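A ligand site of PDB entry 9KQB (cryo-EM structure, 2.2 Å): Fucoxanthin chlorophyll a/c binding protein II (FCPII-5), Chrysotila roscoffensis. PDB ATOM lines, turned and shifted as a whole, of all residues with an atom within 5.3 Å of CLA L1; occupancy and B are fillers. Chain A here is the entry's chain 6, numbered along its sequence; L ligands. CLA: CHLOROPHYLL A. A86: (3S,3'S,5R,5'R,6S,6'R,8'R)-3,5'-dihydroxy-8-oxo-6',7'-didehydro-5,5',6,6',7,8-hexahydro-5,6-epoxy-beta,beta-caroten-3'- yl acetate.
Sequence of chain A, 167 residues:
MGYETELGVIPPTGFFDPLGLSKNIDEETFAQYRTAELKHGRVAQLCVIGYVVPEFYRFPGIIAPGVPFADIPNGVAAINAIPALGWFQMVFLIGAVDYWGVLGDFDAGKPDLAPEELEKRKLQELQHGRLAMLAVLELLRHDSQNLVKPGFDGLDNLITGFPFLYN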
ATOM      1  N   LEU A 134      14.155  28.466  17.108  1.00  0.00           N
ATOM      2  CA  LEU A 134      15.253  27.621  16.645  1.00  0.00           C
ATOM      3  C   LEU A 134      16.576  28.367  16.691  1.00  0.00           C
ATOM      4  O   LEU A 134      17.629  27.761  16.915  1.00  0.00           O
ATOM      5  CB  LEU A 134      14.951  27.116  15.229  1.00  0.00           C
ATOM      6  CG  LEU A 134      13.685  26.267  15.134  1.00  0.00           C
ATOM      7  CD1 LEU A 134      13.393  25.891  13.701  1.00  0.00           C
ATOM      8  CD2 LEU A 134      13.811  25.021  16.010  1.00  0.00           C
ATOM      9  N   LEU A 137      17.637  28.137  20.108  1.00  0.00           N
ATOM     10  CA  LEU A 137      18.038  26.752  20.341  1.00  0.00           C
ATOM     11  C   LEU A 137      19.469  26.490  19.882  1.00  0.00           C
ATOM     12  O   LEU A 137      20.099  25.546  20.363  1.00  0.00           O
ATOM     13  CB  LEU A 137      17.074  25.799  19.652  1.00  0.00           C
ATOM     14  CG  LEU A 137      15.878  25.358  20.496  1.00  0.00           C
ATOM     15  CD1 LEU A 137      14.841  24.642  19.644  1.00  0.00           C
ATOM     16  CD2 LEU A 137      16.328  24.469  21.646  1.00  0.00           C
ATOM     17  N   GLU A 138      19.979  27.286  18.957  1.00  0.00           N
ATOM     18  CA  GLU A 138      21.393  27.253  18.615  1.00  0.00           C
ATOM     19  C   GLU A 138      22.231  28.145  19.527  1.00  0.00           C
ATOM     20  O   GLU A 138      23.408  27.854  19.755  1.00  0.00           O
ATOM     21  CB  GLU A 138      21.616  27.696  17.170  1.00  0.00           C
ATOM     22  CG  GLU A 138      22.853  27.109  16.521  1.00  0.00           C
ATOM     23  CD  GLU A 138      22.516  25.932  15.645  1.00  0.00           C
ATOM     24  OE1 GLU A 138      21.305  25.686  15.471  1.00  0.00           O
ATOM     25  OE2 GLU A 138      23.439  25.273  15.119  1.00  0.00           O
ATOM     26  N   ARG A 141      22.788  26.437  22.734  1.00  0.00           N
ATOM     27  CA  ARG A 141      23.508  25.190  22.458  1.00  0.00           C
ATOM     28  C   ARG A 141      25.007  25.431  22.458  1.00  0.00           C
ATOM     29  O   ARG A 141      25.724  24.907  23.311  1.00  0.00           O
ATOM     30  CB  ARG A 141      23.059  24.616  21.119  1.00  0.00           C
ATOM     31  CG  ARG A 141      23.688  23.269  20.794  1.00  0.00           C
ATOM     32  CD  ARG A 141      23.861  23.071  19.296  1.00  0.00           C
ATOM     33  NE  ARG A 141      24.418  24.255  18.647  1.00  0.00           N
ATOM     34  CZ  ARG A 141      25.608  24.310  18.080  1.00  0.00           C
ATOM     35  NH1 ARG A 141      26.426  23.276  18.074  1.00  0.00           N
ATOM     36  NH2 ARG A 141      26.000  25.446  17.498  1.00  0.00           N
ATOM     37  N   GLN A 145      27.876  24.136  25.232  1.00  0.00           N
ATOM     38  CA  GLN A 145      28.967  23.228  24.896  1.00  0.00           C
ATOM     39  C   GLN A 145      30.309  23.845  25.261  1.00  0.00           C
ATOM     40  O   GLN A 145      31.172  23.193  25.854  1.00  0.00           O
ATOM     41  CB  GLN A 145      28.941  22.864  23.406  1.00  0.00           C
ATOM     42  CG  GLN A 145      27.616  22.366  22.802  1.00  0.00           C
ATOM     43  CD  GLN A 145      27.026  21.084  23.390  1.00  0.00           C
ATOM     44  OE1 GLN A 145      25.972  20.638  22.951  1.00  0.00           O
ATOM     45  NE2 GLN A 145      27.724  20.474  24.348  1.00  0.00           N
ATOM     46  N   PHE A 152      34.790  23.359  22.200  1.00  0.00           N
ATOM     47  CA  PHE A 152      34.228  22.138  21.615  1.00  0.00           C
ATOM     48  C   PHE A 152      34.071  22.288  20.112  1.00  0.00           C
ATOM     49  O   PHE A 152      34.649  21.519  19.329  1.00  0.00           O
ATOM     50  CB  PHE A 152      32.891  21.802  22.272  1.00  0.00           C
ATOM     51  CG  PHE A 152      32.233  20.582  21.717  1.00  0.00           C
ATOM     52  CD1 PHE A 152      32.960  19.416  21.516  1.00  0.00           C
ATOM     53  CD2 PHE A 152      30.883  20.578  21.388  1.00  0.00           C
ATOM     54  CE1 PHE A 152      32.363  18.278  21.002  1.00  0.00           C
ATOM     55  CE2 PHE A 152      30.278  19.450  20.869  1.00  0.00           C
ATOM     56  CZ  PHE A 152      31.021  18.295  20.683  1.00  0.00           C
ATOM     57  N   ASP A 153      33.297  23.279  19.678  1.00  0.00           N
ATOM     58  CA  ASP A 153      33.175  23.570  18.262  1.00  0.00           C
ATOM     59  C   ASP A 153      34.428  24.278  17.772  1.00  0.00           C
ATOM     60  O   ASP A 153      35.305  24.662  18.545  1.00  0.00           O
ATOM     61  CB  ASP A 153      31.934  24.415  17.984  1.00  0.00           C
ATOM     62  CG  ASP A 153      30.679  23.826  18.604  1.00  0.00           C
ATOM     63  OD1 ASP A 153      30.506  23.947  19.835  1.00  0.00           O
ATOM     64  OD2 ASP A 153      29.859  23.230  17.866  1.00  0.00           O
ATOM     65  N   LEU A 155      34.659  27.244  16.421  1.00  0.00           N
ATOM     66  CA  LEU A 155      34.635  28.646  16.816  1.00  0.00           C
ATOM     67  C   LEU A 155      34.394  28.789  18.320  1.00  0.00           C
ATOM     68  O   LEU A 155      33.685  27.998  18.947  1.00  0.00           O
ATOM     69  CB  LEU A 155      33.550  29.403  16.050  1.00  0.00           C
ATOM     70  CG  LEU A 155      32.114  28.906  16.212  1.00  0.00           C
ATOM     71  CD1 LEU A 155      31.141  30.071  16.270  1.00  0.00           C
ATOM     72  CD2 LEU A 155      31.727  27.971  15.084  1.00  0.00           C
HETATM   73 MG   CLA L   1      23.847  23.833  13.621  1.00  0.00          MG
HETATM   74  CHA CLA L   1      26.893  22.518  13.911  1.00  0.00           C
HETATM   75  CHB CLA L   1      22.498  20.807  14.877  1.00  0.00           C
HETATM   76  CHC CLA L   1      20.479  24.692  12.491  1.00  0.00           C
HETATM   77  CHD CLA L   1      24.863  26.992  12.641  1.00  0.00           C
HETATM   78  NA  CLA L   1      24.554  21.923  14.407  1.00  0.00           N
HETATM   79  C1A CLA L   1      25.790  21.649  14.417  1.00  0.00           C
HETATM   80  C2A CLA L   1      26.067  20.289  14.989  1.00  0.00           C
HETATM   81  C3A CLA L   1      24.681  19.684  15.123  1.00  0.00           C
HETATM   82  C4A CLA L   1      23.835  20.865  14.783  1.00  0.00           C
HETATM   83  CMA CLA L   1      24.454  18.562  14.127  1.00  0.00           C
HETATM   84  CAA CLA L   1      26.756  20.361  16.337  1.00  0.00           C
HETATM   85  CBA CLA L   1      27.244  18.973  16.743  1.00  0.00           C
HETATM   86  CGA CLA L   1      28.348  19.108  17.747  1.00  0.00           C
HETATM   87  O1A CLA L   1      28.625  20.195  18.228  1.00  0.00           O
HETATM   88  O2A CLA L   1      29.104  17.933  18.161  1.00  0.00           O
HETATM   89  NB  CLA L   1      21.771  22.730  13.510  1.00  0.00           N
HETATM   90  C1B CLA L   1      21.533  21.886  14.532  1.00  0.00           C
HETATM   91  C2B CLA L   1      20.242  22.118  15.219  1.00  0.00           C
HETATM   92  C3B CLA L   1      19.693  23.272  14.474  1.00  0.00           C
HETATM   93  C4B CLA L   1      20.707  23.567  13.416  1.00  0.00           C
HETATM   94  CMB CLA L   1      19.652  21.383  16.396  1.00  0.00           C
HETATM   95  CAB CLA L   1      18.454  24.071  14.592  1.00  0.00           C
HETATM   96  CBB CLA L   1      18.146  24.645  15.731  1.00  0.00           C
HETATM   97  NC  CLA L   1      22.748  25.574  12.644  1.00  0.00           N
HETATM   98  C1C CLA L   1      21.457  25.806  12.373  1.00  0.00           C
HETATM   99  C2C CLA L   1      21.163  27.204  11.993  1.00  0.00           C
HETATM  100  C3C CLA L   1      22.500  27.839  12.052  1.00  0.00           C
HETATM  101  C4C CLA L   1      23.404  26.736  12.476  1.00  0.00           C
HETATM  102  CMC CLA L   1      19.840  27.832  11.635  1.00  0.00           C
HETATM  103  CAC CLA L   1      22.844  29.283  11.767  1.00  0.00           C
HETATM  104  CBC CLA L   1      23.035  30.043  13.068  1.00  0.00           C
HETATM  105  ND  CLA L   1      25.390  24.714  13.369  1.00  0.00           N
HETATM  106  C1D CLA L   1      25.816  25.878  12.870  1.00  0.00           C
HETATM  107  C2D CLA L   1      27.273  25.906  12.620  1.00  0.00           C
HETATM  108  C3D CLA L   1      27.689  24.546  13.048  1.00  0.00           C
HETATM  109  C4D CLA L   1      26.524  23.894  13.475  1.00  0.00           C
HETATM  110  CMD CLA L   1      28.120  27.022  12.076  1.00  0.00           C
HETATM  111  CAD CLA L   1      28.853  23.636  13.180  1.00  0.00           C
HETATM  112  OBD CLA L   1      30.081  23.896  12.873  1.00  0.00           O
HETATM  113  CBD CLA L   1      28.360  22.378  13.768  1.00  0.00           C
HETATM  114  CGD CLA L   1      28.730  21.200  12.912  1.00  0.00           C
HETATM  115  O1D CLA L   1      29.316  20.265  13.429  1.00  0.00           O
HETATM  116  O2D CLA L   1      28.891  21.345  11.471  1.00  0.00           O
HETATM  117  CED CLA L   1      27.760  21.536  10.619  1.00  0.00           C
HETATM  118 MG   CLA L   2       8.965  32.696   3.520  1.00  0.00          MG
HETATM  119  CHA CLA L   2      10.552  33.044   6.646  1.00  0.00           C
HETATM  120  CHB CLA L   2      11.282  30.225   2.874  1.00  0.00           C
HETATM  121  CHC CLA L   2       7.788  32.796   0.352  1.00  0.00           C
HETATM  122  CHD CLA L   2       6.826  35.573   4.347  1.00  0.00           C
HETATM  123  NA  CLA L   2      10.522  31.590   4.656  1.00  0.00           N
HETATM  124  C1A CLA L   2      10.884  31.835   5.835  1.00  0.00           C
HETATM  125  C2A CLA L   2      11.776  30.783   6.408  1.00  0.00           C
HETATM  126  C3A CLA L   2      12.059  29.899   5.202  1.00  0.00           C
HETATM  127  C4A CLA L   2      11.245  30.586   4.158  1.00  0.00           C
HETATM  128  CMA CLA L   2      13.529  29.928   4.828  1.00  0.00           C
HETATM  129  CAA CLA L   2      11.121  30.074   7.589  1.00  0.00           C
HETATM  130  CBA CLA L   2      10.294  28.843   7.232  1.00  0.00           C
HETATM  131  CGA CLA L   2      10.346  27.908   8.417  1.00  0.00           C
HETATM  132  O1A CLA L   2       9.714  28.155   9.428  1.00  0.00           O
HETATM  133  O2A CLA L   2      11.152  26.687   8.373  1.00  0.00           O
HETATM  134  NB  CLA L   2       9.522  31.708   1.937  1.00  0.00           N
HETATM  135  C1B CLA L   2      10.359  30.653   1.790  1.00  0.00           C
HETATM  136  C2B CLA L   2      10.284  29.992   0.472  1.00  0.00           C
HETATM  137  C3B CLA L   2       9.244  30.797  -0.211  1.00  0.00           C
HETATM  138  C4B CLA L   2       8.831  31.835   0.782  1.00  0.00           C
HETATM  139  CMB CLA L   2      11.052  28.811  -0.045  1.00  0.00           C
HETATM  140  CAB CLA L   2       8.617  30.742  -1.550  1.00  0.00           C
HETATM  141  CBB CLA L   2       9.325  31.059  -2.615  1.00  0.00           C
HETATM  142  NC  CLA L   2       7.501  33.971   2.487  1.00  0.00           N
HETATM  143  C1C CLA L   2       7.212  33.875   1.181  1.00  0.00           C
HETATM  144  C2C CLA L   2       6.285  34.932   0.703  1.00  0.00           C
HETATM  145  C3C CLA L   2       6.027  35.726   1.921  1.00  0.00           C
HETATM  146  C4C CLA L   2       6.827  35.030   2.973  1.00  0.00           C
HETATM  147  CMC CLA L   2       5.737  35.137  -0.693  1.00  0.00           C
HETATM  148  CAC CLA L   2       5.156  36.938   2.083  1.00  0.00           C
HETATM  149  CBC CLA L   2       5.909  38.164   1.628  1.00  0.00           C
HETATM  150  ND  CLA L   2       8.576  34.042   5.074  1.00  0.00           N
HETATM  151  C1D CLA L   2       7.871  35.158   5.301  1.00  0.00           C
HETATM  152  C2D CLA L   2       8.266  35.864   6.535  1.00  0.00           C
HETATM  153  C3D CLA L   2       9.341  34.994   7.058  1.00  0.00           C
HETATM  154  C4D CLA L   2       9.478  33.939   6.151  1.00  0.00           C
HETATM  155  CMD CLA L   2       7.716  37.138   7.105  1.00  0.00           C
HETATM  156  CAD CLA L   2      10.329  34.817   8.157  1.00  0.00           C
HETATM  157  OBD CLA L   2      10.500  35.600   9.167  1.00  0.00           O
HETATM  158  CBD CLA L   2      11.243  33.729   7.743  1.00  0.00           C
HETATM  159  CGD CLA L   2      12.523  34.297   7.199  1.00  0.00           C
HETATM  160  O1D CLA L   2      12.471  35.177   6.357  1.00  0.00           O
HETATM  161  O2D CLA L   2      13.773  34.120   7.931  1.00  0.00           O
HETATM  162  CED CLA L   2      14.317  32.825   8.159  1.00  0.00           C
HETATM  163  C1  CLA L   2      12.553  26.795   8.165  1.00  0.00           C
HETATM  164  C2  CLA L   2      13.334  26.248   9.335  1.00  0.00           C
HETATM  165  C3  CLA L   2      14.645  26.543   9.473  1.00  0.00           C
HETATM  166  C4  CLA L   2      15.343  27.416   8.474  1.00  0.00           C
HETATM  167  C5  CLA L   2      15.426  25.996  10.644  1.00  0.00           C
HETATM  168  C6  CLA L   2      15.420  24.474  10.612  1.00  0.00           C
HETATM  169  C7  CLA L   2      16.634  23.927  11.359  1.00  0.00           C
HETATM  170  C8  CLA L   2      16.604  22.410  11.425  1.00  0.00           C
HETATM  171  C9  CLA L   2      15.598  21.932  12.473  1.00  0.00           C
HETATM  172  C10 CLA L   2      18.013  21.900  11.731  1.00  0.00           C
HETATM  173  C11 CLA L   2      18.044  20.403  11.978  1.00  0.00           C
HETATM  174  C12 CLA L   2      18.663  19.668  10.795  1.00  0.00           C
HETATM  175  C13 CLA L   2      19.987  19.013  11.179  1.00  0.00           C
HETATM  176  C14 CLA L   2      20.635  18.334   9.976  1.00  0.00           C
HETATM  177  C15 CLA L   2      19.757  18.022  12.314  1.00  0.00           C
HETATM  178  C16 CLA L   2      21.081  17.420  12.787  1.00  0.00           C
HETATM  179  C17 CLA L   2      20.843  16.359  13.855  1.00  0.00           C
HETATM  180  C18 CLA L   2      22.141  15.629  14.188  1.00  0.00           C
HETATM  181  C19 CLA L   2      22.709  14.923  12.971  1.00  0.00           C
HETATM  182  C20 CLA L   2      21.937  14.658  15.340  1.00  0.00           C
HETATM  183  C   A86 L   3      12.687  42.174  18.539  1.00  0.00           C
HETATM  184  O   A86 L   3      20.028  33.249  13.525  1.00  0.00           O
HETATM  185  C1  A86 L   3      11.815  41.987  17.359  1.00  0.00           C
HETATM  186  C10 A86 L   3      17.928  35.895  14.318  1.00  0.00           C
HETATM  187  C11 A86 L   3      18.537  34.905  13.636  1.00  0.00           C
HETATM  188  C12 A86 L   3      18.166  34.561  12.245  1.00  0.00           C
HETATM  189  C13 A86 L   3      19.551  34.176  14.190  1.00  0.00           C
HETATM  190  C14 A86 L   3      20.080  34.427  15.579  1.00  0.00           C
HETATM  191  C15 A86 L   3      21.584  34.495  15.727  1.00  0.00           C
HETATM  192  C16 A86 L   3      22.282  35.766  15.191  1.00  0.00           C
HETATM  193  C17 A86 L   3      23.647  35.839  15.890  1.00  0.00           C
HETATM  194  C18 A86 L   3      24.571  34.628  15.758  1.00  0.00           C
HETATM  195  C19 A86 L   3      23.856  33.295  15.610  1.00  0.00           C
HETATM  196  C2  A86 L   3      11.971  40.818  16.596  1.00  0.00           C
HETATM  197  C20 A86 L   3      22.378  33.281  15.947  1.00  0.00           C
HETATM  198  C21 A86 L   3      21.761  31.911  16.023  1.00  0.00           C
HETATM  199  C22 A86 L   3      21.506  36.994  15.675  1.00  0.00           C
HETATM  200  C23 A86 L   3      22.459  35.879  13.675  1.00  0.00           C
HETATM  201  C24 A86 L   3      10.871  42.980  17.068  1.00  0.00           C
HETATM  202  C25 A86 L   3      10.034  43.670  17.942  1.00  0.00           C
HETATM  203  C26 A86 L   3       8.702  43.989  17.761  1.00  0.00           C
HETATM  204  C27 A86 L   3       7.866  44.688  18.634  1.00  0.00           C
HETATM  205  C28 A86 L   3       8.422  45.138  19.935  1.00  0.00           C
HETATM  206  C29 A86 L   3       6.471  45.060  18.367  1.00  0.00           C
HETATM  207  C3  A86 L   3      13.123  40.300  16.035  1.00  0.00           C
HETATM  208  C30 A86 L   3       5.974  46.109  18.950  1.00  0.00           C
HETATM  209  C31 A86 L   3       5.542  47.161  19.589  1.00  0.00           C
HETATM  210  C32 A86 L   3       4.639  47.002  20.816  1.00  0.00           C
HETATM  211  C33 A86 L   3       4.878  48.163  21.810  1.00  0.00           C
HETATM  212  C34 A86 L   3       5.026  49.572  21.244  1.00  0.00           C
HETATM  213  C35 A86 L   3       5.145  49.640  19.737  1.00  0.00           C
HETATM  214  C36 A86 L   3       6.027  48.551  19.149  1.00  0.00           C
HETATM  215  C37 A86 L   3       6.065  48.685  17.633  1.00  0.00           C
HETATM  216  C38 A86 L   3       4.020  51.563  22.144  1.00  0.00           C
HETATM  217  C39 A86 L   3       3.089  52.555  21.557  1.00  0.00           C
HETATM  218  C4  A86 L   3      14.049  39.407  16.529  1.00  0.00           C
HETATM  219  C40 A86 L   3       4.978  45.699  21.541  1.00  0.00           C
HETATM  220  C41 A86 L   3       3.149  46.920  20.427  1.00  0.00           C
HETATM  221  C5  A86 L   3      14.131  38.022  16.442  1.00  0.00           C
HETATM  222  C6  A86 L   3      14.528  37.243  15.336  1.00  0.00           C
HETATM  223  C7  A86 L   3      13.656  37.207  14.142  1.00  0.00           C
HETATM  224  C8  A86 L   3      15.718  36.484  15.323  1.00  0.00           C
HETATM  225  C9  A86 L   3      16.603  36.292  14.266  1.00  0.00           C
HETATM  226  O1  A86 L   3      22.033  34.138  17.058  1.00  0.00           O
HETATM  227  O2  A86 L   3      25.453  34.824  14.647  1.00  0.00           O
HETATM  228  O3  A86 L   3       7.342  48.787  19.675  1.00  0.00           O
HETATM  229  O4  A86 L   3       3.842  50.347  21.590  1.00  0.00           O
HETATM  230  O5  A86 L   3       4.849  51.787  22.980  1.00  0.00           O
HETATM  231 MG   CLA L   4      24.452  18.050  23.169  1.00  0.00          MG
HETATM  232  CHA CLA L   4      27.001  17.023  25.352  1.00  0.00           C
HETATM  233  CHB CLA L   4      25.966  16.808  20.704  1.00  0.00           C
HETATM  234  CHC CLA L   4      21.830  19.510  21.297  1.00  0.00           C
HETATM  235  CHD CLA L   4      23.781  20.938  25.626  1.00  0.00           C
HETATM  236  NA  CLA L   4      26.087  16.912  23.078  1.00  0.00           N
HETATM  237  C1A CLA L   4      26.814  16.425  23.994  1.00  0.00           C
HETATM  238  C2A CLA L   4      27.509  15.175  23.526  1.00  0.00           C
HETATM  239  C3A CLA L   4      27.210  15.137  22.045  1.00  0.00           C
HETATM  240  C4A CLA L   4      26.356  16.356  21.901  1.00  0.00           C
HETATM  241  CMA CLA L   4      28.473  15.279  21.200  1.00  0.00           C
HETATM  242  CAA CLA L   4      27.083  13.914  24.278  1.00  0.00           C
HETATM  243  CBA CLA L   4      25.798  13.271  23.755  1.00  0.00           C
HETATM  244  CGA CLA L   4      24.599  13.952  24.370  1.00  0.00           C
HETATM  245  O1A CLA L   4      23.541  14.011  23.771  1.00  0.00           O
HETATM  246  O2A CLA L   4      24.700  14.542  25.699  1.00  0.00           O
HETATM  247  NB  CLA L   4      24.020  18.192  21.309  1.00  0.00           N
HETATM  248  C1B CLA L   4      24.673  17.470  20.383  1.00  0.00           C
HETATM  249  C2B CLA L   4      23.994  17.422  19.068  1.00  0.00           C
HETATM  250  C3B CLA L   4      22.778  18.234  19.300  1.00  0.00           C
HETATM  251  C4B CLA L   4      22.893  18.663  20.724  1.00  0.00           C
HETATM  252  CMB CLA L   4      24.417  16.711  17.810  1.00  0.00           C
HETATM  253  NC  CLA L   4      22.963  19.977  23.408  1.00  0.00           N
HETATM  254  C1C CLA L   4      22.046  20.348  22.508  1.00  0.00           C
HETATM  255  C2C CLA L   4      21.319  21.585  22.858  1.00  0.00           C
HETATM  256  C3C CLA L   4      21.930  21.959  24.150  1.00  0.00           C
HETATM  257  C4C CLA L   4      22.950  20.894  24.405  1.00  0.00           C
HETATM  258  CMC CLA L   4      20.222  22.292  22.095  1.00  0.00           C
HETATM  259  CAC CLA L   4      21.612  23.153  25.011  1.00  0.00           C
HETATM  260  CBC CLA L   4      20.688  22.739  26.132  1.00  0.00           C
HETATM  261  ND  CLA L   4      25.150  18.993  25.044  1.00  0.00           N
HETATM  262  C1D CLA L   4      24.802  19.921  25.938  1.00  0.00           C
HETATM  263  C2D CLA L   4      25.546  19.796  27.209  1.00  0.00           C
HETATM  264  C3D CLA L   4      26.420  18.622  26.956  1.00  0.00           C
HETATM  265  C4D CLA L   4      26.138  18.193  25.664  1.00  0.00           C
HETATM  266  CMD CLA L   4      25.450  20.642  28.456  1.00  0.00           C
HETATM  267  CAD CLA L   4      27.476  17.754  27.558  1.00  0.00           C
HETATM  268  OBD CLA L   4      27.959  17.881  28.747  1.00  0.00           O
HETATM  269  CBD CLA L   4      27.817  16.721  26.560  1.00  0.00           C
HETATM  270  CGD CLA L   4      29.307  16.715  26.306  1.00  0.00           C
HETATM  271  O1D CLA L   4      30.081  16.884  27.227  1.00  0.00           O
HETATM  272  O2D CLA L   4      29.864  16.917  24.979  1.00  0.00           O
HETATM  273  CED CLA L   4      30.889  16.035  24.506  1.00  0.00           C
HETATM  274 MG   CLA L   5      28.542  36.181   9.270  1.00  0.00          MG
HETATM  275  CHA CLA L   5      31.782  37.062   8.257  1.00  0.00           C
HETATM  276  CHB CLA L   5      29.468  33.125   9.786  1.00  0.00           C
HETATM  277  CHC CLA L   5      25.139  35.625  10.051  1.00  0.00           C
HETATM  278  CHD CLA L   5      27.601  39.826   9.124  1.00  0.00           C
HETATM  279  NA  CLA L   5      30.359  35.199   9.015  1.00  0.00           N
HETATM  280  C1A CLA L   5      31.471  35.641   8.572  1.00  0.00           C
HETATM  281  C2A CLA L   5      32.475  34.546   8.374  1.00  0.00           C
HETATM  282  C3A CLA L   5      31.687  33.293   8.692  1.00  0.00           C
HETATM  283  C4A CLA L   5      30.418  33.884   9.199  1.00  0.00           C
HETATM  284  CMA CLA L   5      31.437  32.445   7.459  1.00  0.00           C
HETATM  285  CAA CLA L   5      33.648  34.680   9.338  1.00  0.00           C
HETATM  286  CBA CLA L   5      34.777  33.706   8.983  1.00  0.00           C
HETATM  287  CGA CLA L   5      35.285  33.993   7.592  1.00  0.00           C
HETATM  288  O1A CLA L   5      35.978  34.973   7.370  1.00  0.00           O
HETATM  289  O2A CLA L   5      34.942  33.110   6.493  1.00  0.00           O
HETATM  290  NB  CLA L   5      27.526  34.656   9.840  1.00  0.00           N
HETATM  291  C1B CLA L   5      28.027  33.419   9.957  1.00  0.00           C
HETATM  292  C2B CLA L   5      27.013  32.389  10.296  1.00  0.00           C
HETATM  293  C3B CLA L   5      25.777  33.178  10.351  1.00  0.00           C
HETATM  294  C4B CLA L   5      26.197  34.574  10.059  1.00  0.00           C
HETATM  295  CMB CLA L   5      27.208  30.904  10.503  1.00  0.00           C
HETATM  296  CAB CLA L   5      24.354  32.849  10.631  1.00  0.00           C
HETATM  297  CBB CLA L   5      23.546  32.522   9.648  1.00  0.00           C
HETATM  298  NC  CLA L   5      26.612  37.512   9.566  1.00  0.00           N
HETATM  299  C1C CLA L   5      25.379  37.067   9.847  1.00  0.00           C
HETATM  300  C2C CLA L   5      24.354  38.136   9.923  1.00  0.00           C
HETATM  301  C3C CLA L   5      25.142  39.353   9.633  1.00  0.00           C
HETATM  302  C4C CLA L   5      26.535  38.856   9.435  1.00  0.00           C
HETATM  303  CMC CLA L   5      22.882  37.993  10.208  1.00  0.00           C
HETATM  304  CAC CLA L   5      24.660  40.787   9.566  1.00  0.00           C
HETATM  305  CBC CLA L   5      23.879  41.015   8.286  1.00  0.00           C
HETATM  306  ND  CLA L   5      29.340  38.109   8.855  1.00  0.00           N
HETATM  307  C1D CLA L   5      28.978  39.400   8.769  1.00  0.00           C
HETATM  308  C2D CLA L   5      30.068  40.275   8.300  1.00  0.00           C
HETATM  309  C3D CLA L   5      31.181  39.324   8.108  1.00  0.00           C
HETATM  310  C4D CLA L   5      30.682  38.052   8.448  1.00  0.00           C
HETATM  311  CMD CLA L   5      30.048  41.765   8.080  1.00  0.00           C
HETATM  312  CAD CLA L   5      32.604  39.198   7.677  1.00  0.00           C
HETATM  313  OBD CLA L   5      33.374  40.162   7.303  1.00  0.00           O
HETATM  314  CBD CLA L   5      32.895  37.754   7.568  1.00  0.00           C
HETATM  315  CGD CLA L   5      32.956  37.340   6.129  1.00  0.00           C
HETATM  316  O1D CLA L   5      31.925  37.025   5.548  1.00  0.00           O
HETATM  317  O2D CLA L   5      34.230  37.142   5.463  1.00  0.00           O
HETATM  318  CED CLA L   5      35.380  37.890   5.865  1.00  0.00           C
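A magnesium atom (MG) of CLA L1 is bound by the side-chain carboxylate of Glu 138, 2.1 Å away. The guanidinium group of Arg 141 lies within salt-bridge range of an oxygen (O1A) of CLA L1, at 3.8 Å.
OE2 of Glu 138 lies close to NH2 of Arg 141, at 3.5 Å. The side-chain carboxylate of Asp 153 is in salt-bridge range of the guanidinium group of Arg 141, at 3.4 Å.
The side-chain carboxylate of Asp 153 sits close to an oxygen (O1A) of CLA L1, 3.3 Å away. O of Leu 134 touches CBB of CLA L1, 3.4 Å away. Phe 152 touches CLA L1 (CZ to O2A, 3.2 Å). Hydrophobic or aromatic side chains that line CLA L1: Phe 152. Five residues have an atom within 4 Å of CLA L1: Leu 134, Glu 138, Arg 141, Phe 152 and Asp 153. The nearest printed residue that does not touch CLA L1 is Leu 137 (4.2 Å).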
